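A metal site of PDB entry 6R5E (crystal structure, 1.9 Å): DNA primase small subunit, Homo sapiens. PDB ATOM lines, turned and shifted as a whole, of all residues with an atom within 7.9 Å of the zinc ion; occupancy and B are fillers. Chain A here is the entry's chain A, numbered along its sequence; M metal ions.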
ATOM      1  N   MET A 115     -16.844  20.055  13.470  1.00  0.00           N
ATOM      2  CA  MET A 115     -16.962  21.217  12.592  1.00  0.00           C
ATOM      3  C   MET A 115     -16.492  22.490  13.299  1.00  0.00           C
ATOM      4  O   MET A 115     -16.088  23.440  12.630  1.00  0.00           O
ATOM      5  CB  MET A 115     -18.404  21.383  12.129  1.00  0.00           C
ATOM      6  CG  MET A 115     -18.539  22.313  10.922  1.00  0.00           C
ATOM      7  SD  MET A 115     -18.444  21.465   9.345  1.00  0.00           S
ATOM      8  CE  MET A 115     -19.979  20.549   9.419  1.00  0.00           C
ATOM      9  N   ARG A 122     -15.371  28.915   8.141  1.00  0.00           N
ATOM     10  CA  ARG A 122     -16.821  28.878   7.979  1.00  0.00           C
ATOM     11  C   ARG A 122     -17.400  30.272   8.190  1.00  0.00           C
ATOM     12  O   ARG A 122     -17.023  30.948   9.145  1.00  0.00           O
ATOM     13  CB  ARG A 122     -17.520  27.954   8.984  1.00  0.00           C
ATOM     14  CG  ARG A 122     -17.173  26.507   9.005  1.00  0.00           C
ATOM     15  CD  ARG A 122     -18.277  25.748   9.762  1.00  0.00           C
ATOM     16  NE  ARG A 122     -18.245  25.936  11.212  1.00  0.00           N
ATOM     17  CZ  ARG A 122     -19.168  25.452  12.042  1.00  0.00           C
ATOM     18  NH1 ARG A 122     -20.196  24.768  11.567  1.00  0.00           N
ATOM     19  NH2 ARG A 122     -19.062  25.652  13.348  1.00  0.00           N
ATOM     20  N   ARG A 123     -18.348  30.677   7.336  1.00  0.00           N
ATOM     21  CA  ARG A 123     -19.051  31.943   7.527  1.00  0.00           C
ATOM     22  C   ARG A 123     -20.471  31.769   8.052  1.00  0.00           C
ATOM     23  O   ARG A 123     -21.020  32.726   8.619  1.00  0.00           O
ATOM     24  CB  ARG A 123     -19.107  32.735   6.224  1.00  0.00           C
ATOM     25  CG  ARG A 123     -17.760  33.268   5.733  1.00  0.00           C
ATOM     26  CD  ARG A 123     -17.930  34.098   4.470  1.00  0.00           C
ATOM     27  NE  ARG A 123     -18.730  35.311   4.694  1.00  0.00           N
ATOM     28  CZ  ARG A 123     -19.405  35.953   3.752  1.00  0.00           C
ATOM     29  NH1 ARG A 123     -19.410  35.515   2.498  1.00  0.00           N
ATOM     30  NH2 ARG A 123     -20.090  37.051   4.065  1.00  0.00           N
ATOM     31  N   CYS A 124     -21.082  30.597   7.871  1.00  0.00           N
ATOM     32  CA  CYS A 124     -22.490  30.412   8.196  1.00  0.00           C
ATOM     33  C   CYS A 124     -22.720  30.096   9.667  1.00  0.00           C
ATOM     34  O   CYS A 124     -23.713  30.554  10.255  1.00  0.00           O
ATOM     35  CB  CYS A 124     -23.051  29.292   7.326  1.00  0.00           C
ATOM     36  SG  CYS A 124     -21.989  27.823   7.338  1.00  0.00           S
ATOM     37  N   CYS A 125     -21.822  29.337  10.285  1.00  0.00           N
ATOM     38  CA  CYS A 125     -22.019  28.805  11.621  1.00  0.00           C
ATOM     39  C   CYS A 125     -20.757  29.001  12.457  1.00  0.00           C
ATOM     40  O   CYS A 125     -19.671  29.221  11.919  1.00  0.00           O
ATOM     41  CB  CYS A 125     -22.361  27.307  11.605  1.00  0.00           C
ATOM     42  SG  CYS A 125     -23.867  26.834  10.733  1.00  0.00           S
ATOM     43  N   SER A 126     -20.922  28.902  13.767  1.00  0.00           N
ATOM     44  CA  SER A 126     -19.805  28.862  14.691  1.00  0.00           C
ATOM     45  C   SER A 126     -20.142  27.939  15.851  1.00  0.00           C
ATOM     46  O   SER A 126     -21.293  27.546  16.050  1.00  0.00           O
ATOM     47  CB  SER A 126     -19.445  30.262  15.222  1.00  0.00           C
ATOM     48  OG  SER A 126     -20.479  30.788  16.026  1.00  0.00           O
ATOM     49  N   ASP A 129     -22.783  24.702  16.190  1.00  0.00           N
ATOM     50  CA  ASP A 129     -23.789  24.756  15.143  1.00  0.00           C
ATOM     51  C   ASP A 129     -23.266  24.120  13.864  1.00  0.00           C
ATOM     52  O   ASP A 129     -22.070  24.177  13.550  1.00  0.00           O
ATOM     53  CB  ASP A 129     -24.207  26.193  14.859  1.00  0.00           C
ATOM     54  CG  ASP A 129     -25.065  26.782  15.965  1.00  0.00           C
ATOM     55  OD1 ASP A 129     -25.741  26.004  16.677  1.00  0.00           O
ATOM     56  OD2 ASP A 129     -25.084  28.024  16.114  1.00  0.00           O
ATOM     57  N   ILE A 130     -24.188  23.513  13.109  1.00  0.00           N
ATOM     58  CA  ILE A 130     -23.926  23.039  11.757  1.00  0.00           C
ATOM     59  C   ILE A 130     -25.133  23.376  10.904  1.00  0.00           C
ATOM     60  O   ILE A 130     -26.235  23.619  11.421  1.00  0.00           O
ATOM     61  CB  ILE A 130     -23.617  21.520  11.695  1.00  0.00           C
ATOM     62  CG1 ILE A 130     -24.837  20.701  12.136  1.00  0.00           C
ATOM     63  CG2 ILE A 130     -22.409  21.194  12.556  1.00  0.00           C
ATOM     64  CD1 ILE A 130     -24.662  19.186  11.980  1.00  0.00           C
ATOM     65  N   CYS A 131     -24.939  23.401   9.600  1.00  0.00           N
ATOM     66  CA  CYS A 131     -26.025  23.666   8.669  1.00  0.00           C
ATOM     67  C   CYS A 131     -25.658  23.075   7.324  1.00  0.00           C
ATOM     68  O   CYS A 131     -24.513  22.642   7.113  1.00  0.00           O
ATOM     69  CB  CYS A 131     -26.318  25.178   8.551  1.00  0.00           C
ATOM     70  SG  CYS A 131     -25.263  26.048   7.367  1.00  0.00           S
ATOM     71  N   PRO A 132     -26.601  23.022   6.377  1.00  0.00           N
ATOM     72  CA  PRO A 132     -26.312  22.405   5.076  1.00  0.00           C
ATOM     73  C   PRO A 132     -25.251  23.147   4.270  1.00  0.00           C
ATOM     74  O   PRO A 132     -24.666  22.554   3.365  1.00  0.00           O
ATOM     75  CB  PRO A 132     -27.670  22.407   4.363  1.00  0.00           C
ATOM     76  CG  PRO A 132     -28.682  22.559   5.472  1.00  0.00           C
ATOM     77  CD  PRO A 132     -28.017  23.414   6.502  1.00  0.00           C
ATOM     78  N   LYS A 133     -25.000  24.417   4.570  1.00  0.00           N
ATOM     79  CA  LYS A 133     -24.022  25.182   3.789  1.00  0.00           C
ATOM     80  C   LYS A 133     -22.591  24.905   4.233  1.00  0.00           C
ATOM     81  O   LYS A 133     -21.666  25.243   3.482  1.00  0.00           O
ATOM     82  CB  LYS A 133     -24.312  26.681   3.902  1.00  0.00           C
ATOM     83  CG  LYS A 133     -25.726  27.060   3.486  1.00  0.00           C
ATOM     84  CD  LYS A 133     -26.092  28.449   3.962  1.00  0.00           C
ATOM     85  CE  LYS A 133     -25.700  29.523   2.969  1.00  0.00           C
ATOM     86  NZ  LYS A 133     -26.054  30.869   3.492  1.00  0.00           N
ATOM     87  N   CYS A 134     -22.382  24.315   5.411  1.00  0.00           N
ATOM     88  CA  CYS A 134     -21.053  23.906   5.842  1.00  0.00           C
ATOM     89  C   CYS A 134     -20.899  22.404   6.001  1.00  0.00           C
ATOM     90  O   CYS A 134     -19.764  21.928   6.135  1.00  0.00           O
ATOM     91  CB  CYS A 134     -20.671  24.598   7.168  1.00  0.00           C
ATOM     92  SG  CYS A 134     -21.786  24.365   8.582  1.00  0.00           S
ATOM     93  N   TRP A 135     -21.990  21.625   5.986  1.00  0.00           N
ATOM     94  CA  TRP A 135     -21.837  20.187   6.156  1.00  0.00           C
ATOM     95  C   TRP A 135     -20.965  19.564   5.074  1.00  0.00           C
ATOM     96  O   TRP A 135     -20.353  18.514   5.302  1.00  0.00           O
ATOM     97  CB  TRP A 135     -23.200  19.476   6.171  1.00  0.00           C
ATOM     98  CG  TRP A 135     -23.020  18.024   6.430  1.00  0.00           C
ATOM     99  CD1 TRP A 135     -23.106  17.014   5.521  1.00  0.00           C
ATOM    100  CD2 TRP A 135     -22.670  17.418   7.682  1.00  0.00           C
ATOM    101  NE1 TRP A 135     -22.840  15.806   6.133  1.00  0.00           N
ATOM    102  CE2 TRP A 135     -22.565  16.032   7.456  1.00  0.00           C
ATOM    103  CE3 TRP A 135     -22.435  17.909   8.966  1.00  0.00           C
ATOM    104  CZ2 TRP A 135     -22.246  15.127   8.468  1.00  0.00           C
ATOM    105  CZ3 TRP A 135     -22.116  17.005   9.978  1.00  0.00           C
ATOM    106  CH2 TRP A 135     -22.023  15.633   9.721  1.00  0.00           C
ATOM    107  N   LEU A 137     -18.142  20.297   4.323  1.00  0.00           N
ATOM    108  CA  LEU A 137     -16.808  20.084   4.893  1.00  0.00           C
ATOM    109  C   LEU A 137     -16.652  18.643   5.375  1.00  0.00           C
ATOM    110  O   LEU A 137     -15.581  18.040   5.214  1.00  0.00           O
ATOM    111  CB  LEU A 137     -16.560  21.052   6.043  1.00  0.00           C
ATOM    112  CG  LEU A 137     -16.252  22.519   5.718  1.00  0.00           C
ATOM    113  CD1 LEU A 137     -16.278  23.318   7.006  1.00  0.00           C
ATOM    114  CD2 LEU A 137     -14.916  22.660   5.021  1.00  0.00           C
ATOM    115  N   TYR A 229     -19.263  24.697  -2.915  1.00  0.00           N
ATOM    116  CA  TYR A 229     -19.121  24.903  -1.473  1.00  0.00           C
ATOM    117  C   TYR A 229     -18.526  26.265  -1.157  1.00  0.00           C
ATOM    118  O   TYR A 229     -19.130  27.079  -0.445  1.00  0.00           O
ATOM    119  CB  TYR A 229     -18.258  23.802  -0.845  1.00  0.00           C
ATOM    120  CG  TYR A 229     -17.874  24.202   0.556  1.00  0.00           C
ATOM    121  CD1 TYR A 229     -18.822  24.234   1.568  1.00  0.00           C
ATOM    122  CD2 TYR A 229     -16.575  24.601   0.854  1.00  0.00           C
ATOM    123  CE1 TYR A 229     -18.493  24.635   2.846  1.00  0.00           C
ATOM    124  CE2 TYR A 229     -16.232  24.997   2.140  1.00  0.00           C
ATOM    125  CZ  TYR A 229     -17.196  25.022   3.126  1.00  0.00           C
ATOM    126  OH  TYR A 229     -16.877  25.409   4.398  1.00  0.00           O
ATOM    127  N   GLN A 234     -20.424  29.363   0.563  1.00  0.00           N
ATOM    128  CA  GLN A 234     -19.684  30.177   1.521  1.00  0.00           C
ATOM    129  C   GLN A 234     -19.345  31.563   0.974  1.00  0.00           C
ATOM    130  O   GLN A 234     -19.134  32.487   1.765  1.00  0.00           O
ATOM    131  CB  GLN A 234     -18.396  29.475   1.943  1.00  0.00           C
ATOM    132  CG  GLN A 234     -18.600  28.239   2.827  1.00  0.00           C
ATOM    133  CD  GLN A 234     -19.282  28.557   4.150  1.00  0.00           C
ATOM    134  OE1 GLN A 234     -18.954  29.548   4.807  1.00  0.00           O
ATOM    135  NE2 GLN A 234     -20.238  27.729   4.541  1.00  0.00           N
ATOM    136  N   PHE A 348     -29.943  16.630   9.547  1.00  0.00           N
ATOM    137  CA  PHE A 348     -31.211  17.071  10.088  1.00  0.00           C
ATOM    138  C   PHE A 348     -32.361  16.100   9.820  1.00  0.00           C
ATOM    139  O   PHE A 348     -33.455  16.314  10.341  1.00  0.00           O
ATOM    140  CB  PHE A 348     -31.542  18.458   9.542  1.00  0.00           C
ATOM    141  CG  PHE A 348     -30.582  19.507   9.997  1.00  0.00           C
ATOM    142  CD1 PHE A 348     -30.773  20.148  11.208  1.00  0.00           C
ATOM    143  CD2 PHE A 348     -29.446  19.788   9.269  1.00  0.00           C
ATOM    144  CE1 PHE A 348     -29.865  21.088  11.653  1.00  0.00           C
ATOM    145  CE2 PHE A 348     -28.530  20.729   9.703  1.00  0.00           C
ATOM    146  CZ  PHE A 348     -28.738  21.374  10.896  1.00  0.00           C
HETATM  147 ZN    ZN M   1     -23.182  26.284   8.544  1.00  0.00          ZN
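The zinc ion is bound by the side-chain sulfur (SG) of Cys 124 (2.3 Å), the side-chain sulfur (SG) of Cys 125 (2.4 Å), the side-chain sulfur (SG) of Cys 134 (2.4 Å) and the side-chain sulfur (SG) of Cys 131 (2.4 Å).
The side-chain sulfur (SG) of Cys 131 lies close to the backbone NH (N) of Lys 133 (3.2 Å).
The side-chain sulfur (SG) of Cys 134 sits close to the guanidinium group (NH1) of Arg 122 (3.4 Å).
The side-chain sulfur (SG) of Cys 124 lies close to the side-chain amide nitrogen (NE2) of Gln 234, 3.3 Å away.
Within 4 Å of the zinc ion: Cys 124, Cys 125, Cys 131 and Cys 134.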
